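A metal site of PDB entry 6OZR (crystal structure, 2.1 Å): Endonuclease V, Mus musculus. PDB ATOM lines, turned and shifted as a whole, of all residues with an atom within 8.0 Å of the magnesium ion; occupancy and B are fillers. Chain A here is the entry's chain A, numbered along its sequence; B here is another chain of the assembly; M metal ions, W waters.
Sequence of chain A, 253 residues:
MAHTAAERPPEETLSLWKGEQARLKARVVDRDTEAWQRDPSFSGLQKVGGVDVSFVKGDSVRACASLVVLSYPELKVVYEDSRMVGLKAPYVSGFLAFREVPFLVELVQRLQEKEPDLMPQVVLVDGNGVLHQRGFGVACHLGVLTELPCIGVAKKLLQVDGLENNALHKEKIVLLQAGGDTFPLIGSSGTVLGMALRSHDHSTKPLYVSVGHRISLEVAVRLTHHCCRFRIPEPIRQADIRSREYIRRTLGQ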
ATOM      1  N   VAL A  51      20.739  -3.223   8.048  1.00  0.00           N
ATOM      2  CA  VAL A  51      19.976  -4.282   8.693  1.00  0.00           C
ATOM      3  C   VAL A  51      20.836  -4.981   9.742  1.00  0.00           C
ATOM      4  O   VAL A  51      22.063  -5.062   9.605  1.00  0.00           O
ATOM      5  CB  VAL A  51      19.444  -5.318   7.676  1.00  0.00           C
ATOM      6  CG1 VAL A  51      18.370  -4.697   6.807  1.00  0.00           C
ATOM      7  CG2 VAL A  51      20.556  -5.851   6.820  1.00  0.00           C
ATOM      8  N   ASP A  52      20.175  -5.509  10.772  1.00  0.00           N
ATOM      9  CA  ASP A  52      20.805  -6.342  11.779  1.00  0.00           C
ATOM     10  C   ASP A  52      19.774  -7.323  12.322  1.00  0.00           C
ATOM     11  O   ASP A  52      18.583  -6.993  12.434  1.00  0.00           O
ATOM     12  CB  ASP A  52      21.372  -5.496  12.940  1.00  0.00           C
ATOM     13  CG  ASP A  52      21.931  -6.359  14.070  1.00  0.00           C
ATOM     14  OD1 ASP A  52      23.036  -6.910  13.911  1.00  0.00           O
ATOM     15  OD2 ASP A  52      21.258  -6.476  15.120  1.00  0.00           O
ATOM     16  N   VAL A  53      20.224  -8.527  12.666  1.00  0.00           N
ATOM     17  CA  VAL A  53      19.397  -9.506  13.367  1.00  0.00           C
ATOM     18  C   VAL A  53      20.177  -9.966  14.582  1.00  0.00           C
ATOM     19  O   VAL A  53      21.179 -10.668  14.452  1.00  0.00           O
ATOM     20  CB  VAL A  53      19.006 -10.687  12.467  1.00  0.00           C
ATOM     21  CG1 VAL A  53      18.055 -11.600  13.201  1.00  0.00           C
ATOM     22  CG2 VAL A  53      18.360 -10.186  11.161  1.00  0.00           C
ATOM     23  N   SER A  54      19.703  -9.596  15.765  1.00  0.00           N
ATOM     24  CA  SER A  54      20.325  -9.958  17.022  1.00  0.00           C
ATOM     25  C   SER A  54      19.477 -11.015  17.726  1.00  0.00           C
ATOM     26  O   SER A  54      18.249 -10.904  17.767  1.00  0.00           O
ATOM     27  CB  SER A  54      20.497  -8.737  17.911  1.00  0.00           C
ATOM     28  OG  SER A  54      20.639  -9.118  19.260  1.00  0.00           O
ATOM     29  N   VAL A 125      24.449  -4.691   4.511  1.00  0.00           N
ATOM     30  CA  VAL A 125      24.027  -5.918   5.181  1.00  0.00           C
ATOM     31  C   VAL A 125      25.153  -6.410   6.076  1.00  0.00           C
ATOM     32  O   VAL A 125      26.316  -6.419   5.677  1.00  0.00           O
ATOM     33  CB  VAL A 125      23.629  -6.997   4.158  1.00  0.00           C
ATOM     34  CG1 VAL A 125      23.059  -8.233   4.855  1.00  0.00           C
ATOM     35  CG2 VAL A 125      22.626  -6.438   3.140  1.00  0.00           C
ATOM     36  N   ASP A 126      24.796  -6.824   7.304  1.00  0.00           N
ATOM     37  CA  ASP A 126      25.702  -7.476   8.251  1.00  0.00           C
ATOM     38  C   ASP A 126      26.076  -8.873   7.769  1.00  0.00           C
ATOM     39  O   ASP A 126      25.337  -9.823   8.023  1.00  0.00           O
ATOM     40  CB  ASP A 126      25.009  -7.627   9.600  1.00  0.00           C
ATOM     41  CG  ASP A 126      25.553  -6.720  10.642  1.00  0.00           C
ATOM     42  OD1 ASP A 126      26.795  -6.604  10.749  1.00  0.00           O
ATOM     43  OD2 ASP A 126      24.723  -6.137  11.380  1.00  0.00           O
ATOM     44  N   GLY A 127      27.204  -9.022   7.077  1.00  0.00           N
ATOM     45  CA  GLY A 127      27.582 -10.313   6.515  1.00  0.00           C
ATOM     46  C   GLY A 127      27.999 -10.191   5.060  1.00  0.00           C
ATOM     47  O   GLY A 127      27.670  -9.188   4.422  1.00  0.00           O
ATOM     48  N   VAL A 153      28.983  -6.274   4.378  1.00  0.00           N
ATOM     49  CA  VAL A 153      29.990  -5.762   5.320  1.00  0.00           C
ATOM     50  C   VAL A 153      30.185  -6.805   6.425  1.00  0.00           C
ATOM     51  O   VAL A 153      29.239  -7.137   7.157  1.00  0.00           O
ATOM     52  CB  VAL A 153      29.575  -4.411   5.926  1.00  0.00           C
ATOM     53  CG1 VAL A 153      30.682  -3.860   6.807  1.00  0.00           C
ATOM     54  CG2 VAL A 153      29.238  -3.391   4.815  1.00  0.00           C
ATOM     55  N   LYS A 155      32.796  -8.318   9.724  1.00  0.00           N
ATOM     56  CA  LYS A 155      33.732  -7.863  10.754  1.00  0.00           C
ATOM     57  C   LYS A 155      34.928  -8.785  10.960  1.00  0.00           C
ATOM     58  O   LYS A 155      35.813  -8.445  11.751  1.00  0.00           O
ATOM     59  CB  LYS A 155      32.987  -7.673  12.081  1.00  0.00           C
ATOM     60  CG  LYS A 155      31.919  -6.593  11.992  1.00  0.00           C
ATOM     61  CD  LYS A 155      31.112  -6.525  13.276  1.00  0.00           C
ATOM     62  CE  LYS A 155      30.187  -7.697  13.393  1.00  0.00           C
ATOM     63  NZ  LYS A 155      29.034  -7.617  12.462  1.00  0.00           N
ATOM     64  N   ILE A 232      32.011   0.346  12.675  1.00  0.00           N
ATOM     65  CA  ILE A 232      30.838  -0.243  12.019  1.00  0.00           C
ATOM     66  C   ILE A 232      30.105   0.862  11.253  1.00  0.00           C
ATOM     67  O   ILE A 232      29.768   1.895  11.854  1.00  0.00           O
ATOM     68  CB  ILE A 232      29.922  -0.890  13.051  1.00  0.00           C
ATOM     69  CG1 ILE A 232      30.706  -1.917  13.871  1.00  0.00           C
ATOM     70  CG2 ILE A 232      28.684  -1.532  12.372  1.00  0.00           C
ATOM     71  CD1 ILE A 232      31.400  -2.941  13.010  1.00  0.00           C
ATOM     72  N   ILE A 236      24.370   0.098   9.625  1.00  0.00           N
ATOM     73  CA  ILE A 236      24.396  -1.160  10.380  1.00  0.00           C
ATOM     74  C   ILE A 236      24.472  -0.874  11.874  1.00  0.00           C
ATOM     75  O   ILE A 236      23.793  -1.528  12.679  1.00  0.00           O
ATOM     76  CB  ILE A 236      25.560  -2.049   9.928  1.00  0.00           C
ATOM     77  CG1 ILE A 236      25.305  -2.568   8.506  1.00  0.00           C
ATOM     78  CG2 ILE A 236      25.738  -3.213  10.882  1.00  0.00           C
ATOM     79  CD1 ILE A 236      26.528  -3.260   7.922  1.00  0.00           C
ATOM     80  N   ARG A 237      25.311   0.084  12.259  1.00  0.00           N
ATOM     81  CA  ARG A 237      25.479   0.408  13.670  1.00  0.00           C
ATOM     82  C   ARG A 237      24.161   0.828  14.312  1.00  0.00           C
ATOM     83  O   ARG A 237      23.818   0.379  15.398  1.00  0.00           O
ATOM     84  CB  ARG A 237      26.536   1.498  13.824  1.00  0.00           C
ATOM     85  CG  ARG A 237      26.848   1.839  15.274  1.00  0.00           C
ATOM     86  CD  ARG A 237      27.953   2.880  15.369  1.00  0.00           C
ATOM     87  NE  ARG A 237      28.058   3.368  16.750  1.00  0.00           N
ATOM     88  CZ  ARG A 237      27.538   4.513  17.169  1.00  0.00           C
ATOM     89  NH1 ARG A 237      26.904   5.310  16.306  1.00  0.00           N
ATOM     90  NH2 ARG A 237      27.663   4.855  18.442  1.00  0.00           N
ATOM     91  N   ALA A 239      21.120   0.060  13.291  1.00  0.00           N
ATOM     92  CA  ALA A 239      20.229  -1.084  13.377  1.00  0.00           C
ATOM     93  C   ALA A 239      20.641  -2.018  14.519  1.00  0.00           C
ATOM     94  O   ALA A 239      19.779  -2.594  15.201  1.00  0.00           O
ATOM     95  CB  ALA A 239      20.188  -1.826  12.036  1.00  0.00           C
ATOM     96  N   ASP A 240      21.965  -2.192  14.739  1.00  0.00           N
ATOM     97  CA  ASP A 240      22.461  -2.947  15.899  1.00  0.00           C
ATOM     98  C   ASP A 240      21.937  -2.362  17.199  1.00  0.00           C
ATOM     99  O   ASP A 240      21.408  -3.075  18.056  1.00  0.00           O
ATOM    100  CB  ASP A 240      24.005  -2.914  15.966  1.00  0.00           C
ATOM    101  CG  ASP A 240      24.680  -3.638  14.817  1.00  0.00           C
ATOM    102  OD1 ASP A 240      24.021  -4.418  14.120  1.00  0.00           O
ATOM    103  OD2 ASP A 240      25.909  -3.416  14.625  1.00  0.00           O
ATOM    104  N   ILE A 241      22.134  -1.049  17.375  1.00  0.00           N
ATOM    105  CA  ILE A 241      21.715  -0.377  18.595  1.00  0.00           C
ATOM    106  C   ILE A 241      20.242  -0.615  18.863  1.00  0.00           C
ATOM    107  O   ILE A 241      19.846  -0.923  19.988  1.00  0.00           O
ATOM    108  CB  ILE A 241      22.054   1.121  18.493  1.00  0.00           C
ATOM    109  CG1 ILE A 241      23.579   1.314  18.517  1.00  0.00           C
ATOM    110  CG2 ILE A 241      21.369   1.911  19.603  1.00  0.00           C
ATOM    111  CD1 ILE A 241      23.999   2.752  18.371  1.00  0.00           C
ATOM    112  N   SER A 243      18.304  -3.110  17.653  1.00  0.00           N
ATOM    113  CA  SER A 243      18.051  -4.514  17.965  1.00  0.00           C
ATOM    114  C   SER A 243      18.339  -4.818  19.437  1.00  0.00           C
ATOM    115  O   SER A 243      17.526  -5.450  20.118  1.00  0.00           O
ATOM    116  CB  SER A 243      18.880  -5.415  17.058  1.00  0.00           C
ATOM    117  OG  SER A 243      18.287  -5.520  15.785  1.00  0.00           O
ATOM    118  N   ARG A 244      19.488  -4.362  19.941  1.00  0.00           N
ATOM    119  CA  ARG A 244      19.849  -4.643  21.324  1.00  0.00           C
ATOM    120  C   ARG A 244      18.938  -3.910  22.301  1.00  0.00           C
ATOM    121  O   ARG A 244      18.527  -4.483  23.323  1.00  0.00           O
ATOM    122  CB  ARG A 244      21.316  -4.292  21.565  1.00  0.00           C
ATOM    123  CG  ARG A 244      22.286  -5.130  20.718  1.00  0.00           C
ATOM    124  CD  ARG A 244      23.738  -5.000  21.153  1.00  0.00           C
ATOM    125  NE  ARG A 244      24.276  -3.650  20.992  1.00  0.00           N
ATOM    126  CZ  ARG A 244      24.967  -3.230  19.938  1.00  0.00           C
ATOM    127  NH1 ARG A 244      25.195  -4.059  18.925  1.00  0.00           N
ATOM    128  NH2 ARG A 244      25.429  -1.985  19.883  1.00  0.00           N
ATOM    129  P     A B  11      30.793 -11.475  10.970  1.00  0.00           P
ATOM    130  OP1   A B  11      30.867 -10.046  10.608  1.00  0.00           O
ATOM    131  OP2   A B  11      31.544 -11.971  12.149  1.00  0.00           O
ATOM    132  O5'   A B  11      29.265 -11.891  11.170  1.00  0.00           O
ATOM    133  C5'   A B  11      28.253 -11.428  10.298  1.00  0.00           C
ATOM    134  C4'   A B  11      26.900 -12.008  10.686  1.00  0.00           C
ATOM    135  O4'   A B  11      26.953 -13.461  10.607  1.00  0.00           O
ATOM    136  C3'   A B  11      26.435 -11.733  12.103  1.00  0.00           C
ATOM    137  O3'   A B  11      25.857 -10.454  12.234  1.00  0.00           O
ATOM    138  C2'   A B  11      25.470 -12.872  12.352  1.00  0.00           C
ATOM    139  O2'   A B  11      24.224 -12.635  11.704  1.00  0.00           O
ATOM    140  C1'   A B  11      26.166 -14.021  11.631  1.00  0.00           C
ATOM    141  N9    A B  11      27.037 -14.807  12.528  1.00  0.00           N
ATOM    142  C8    A B  11      28.410 -14.796  12.569  1.00  0.00           C
ATOM    143  N7    A B  11      28.898 -15.622  13.474  1.00  0.00           N
ATOM    144  C5    A B  11      27.783 -16.192  14.065  1.00  0.00           C
ATOM    145  C6    A B  11      27.635 -17.153  15.086  1.00  0.00           C
ATOM    146  N6    A B  11      28.670 -17.713  15.723  1.00  0.00           N
ATOM    147  N1    A B  11      26.380 -17.505  15.432  1.00  0.00           N
ATOM    148  C2    A B  11      25.354 -16.941  14.791  1.00  0.00           C
ATOM    149  N3    A B  11      25.368 -16.037  13.806  1.00  0.00           N
ATOM    150  C4    A B  11      26.628 -15.700  13.488  1.00  0.00           C
ATOM    151  P     U B  12      26.244  -9.512  13.472  1.00  0.00           P
ATOM    152  OP1   U B  12      25.446  -8.264  13.321  1.00  0.00           O
ATOM    153  OP2   U B  12      27.709  -9.450  13.617  1.00  0.00           O
ATOM    154  O5'   U B  12      25.697 -10.308  14.739  1.00  0.00           O
ATOM    155  C5'   U B  12      24.317 -10.592  14.842  1.00  0.00           C
ATOM    156  C4'   U B  12      24.047 -11.648  15.889  1.00  0.00           C
ATOM    157  O4'   U B  12      24.716 -12.892  15.531  1.00  0.00           O
ATOM    158  C3'   U B  12      24.583 -11.331  17.281  1.00  0.00           C
ATOM    159  O3'   U B  12      23.739 -10.459  18.002  1.00  0.00           O
ATOM    160  C2'   U B  12      24.701 -12.712  17.900  1.00  0.00           C
ATOM    161  O2'   U B  12      23.424 -13.168  18.274  1.00  0.00           O
ATOM    162  C1'   U B  12      25.168 -13.540  16.710  1.00  0.00           C
ATOM    163  N1    U B  12      26.646 -13.686  16.641  1.00  0.00           N
ATOM    164  C2    U B  12      27.265 -14.629  17.463  1.00  0.00           C
ATOM    165  O2    U B  12      26.637 -15.313  18.241  1.00  0.00           O
ATOM    166  N3    U B  12      28.637 -14.720  17.329  1.00  0.00           N
ATOM    167  C4    U B  12      29.425 -13.969  16.469  1.00  0.00           C
ATOM    168  O4    U B  12      30.648 -14.142  16.430  1.00  0.00           O
ATOM    169  C5    U B  12      28.721 -13.025  15.669  1.00  0.00           C
ATOM    170  C6    U B  12      27.392 -12.929  15.770  1.00  0.00           C
ATOM    171  P     A B  13      24.378  -9.524  19.126  1.00  0.00           P
ATOM    172  OP1   A B  13      23.396  -8.499  19.550  1.00  0.00           O
ATOM    173  OP2   A B  13      25.699  -9.093  18.608  1.00  0.00           O
ATOM    174  O5'   A B  13      24.628 -10.531  20.337  1.00  0.00           O
ATOM    175  C5'   A B  13      23.553 -11.250  20.941  1.00  0.00           C
ATOM    176  C4'   A B  13      24.046 -12.372  21.828  1.00  0.00           C
ATOM    177  O4'   A B  13      24.783 -13.346  21.026  1.00  0.00           O
ATOM    178  C3'   A B  13      25.030 -11.974  22.918  1.00  0.00           C
ATOM    179  O3'   A B  13      24.408 -11.412  24.067  1.00  0.00           O
ATOM    180  C2'   A B  13      25.772 -13.273  23.174  1.00  0.00           C
ATOM    181  O2'   A B  13      24.960 -14.178  23.921  1.00  0.00           O
ATOM    182  C1'   A B  13      25.895 -13.824  21.765  1.00  0.00           C
ATOM    183  N9    A B  13      27.134 -13.371  21.107  1.00  0.00           N
ATOM    184  C8    A B  13      27.262 -12.288  20.257  1.00  0.00           C
ATOM    185  N7    A B  13      28.482 -12.112  19.808  1.00  0.00           N
ATOM    186  C5    A B  13      29.211 -13.134  20.404  1.00  0.00           C
ATOM    187  C6    A B  13      30.577 -13.476  20.314  1.00  0.00           C
ATOM    188  N6    A B  13      31.463 -12.806  19.561  1.00  0.00           N
ATOM    189  N1    A B  13      30.995 -14.528  21.041  1.00  0.00           N
ATOM    190  C2    A B  13      30.094 -15.203  21.776  1.00  0.00           C
ATOM    191  N3    A B  13      28.791 -14.975  21.930  1.00  0.00           N
ATOM    192  C4    A B  13      28.406 -13.909  21.215  1.00  0.00           C
HETATM  193 MG    MG M   1      24.998  -6.409  13.876  1.00  0.00          MG
HETATM  194  O   HOH W   1      26.689  -5.501  13.407  1.00  0.00           O
HETATM  195  O   HOH W   2      24.972  -6.975  15.867  1.00  0.00           O
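Of the 20 residues printed, 4 come within 4 Å of the magnesium ion.
Water W1 lies within hydrogen-bond range of OD2 of Asp 240 (2.5 Å), OD1 of Asp 126 (2.9 Å) and NZ of Lys 155 (3.3 Å).
The side-chain hydroxyl of Ser 243 is in hydrogen-bond range of the side-chain carboxylate of Asp 52 (3.2 Å). OP2 of U 12 of chain B lies within salt-bridge range of NZ of Lys 155. The side-chain amino group (NZ) of Lys 155 is in salt-bridge range of the side-chain carboxylate (OD1) of Asp 126 (3.0 Å).
Water W1 binds the magnesium ion (2.0 Å). OP1 of U 12 of chain B is bound to the magnesium ion (2.0 Å). The magnesium ion is bound by OD1 of Asp 52, 2.0 Å away. Water W2 is bound to the magnesium ion. The side-chain carboxylate (OD1) of Asp 240 is bound to the magnesium ion, 2.2 Å away. The side-chain carboxylate (OD2) of Asp 126 binds the magnesium ion, at 2.5 Å.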
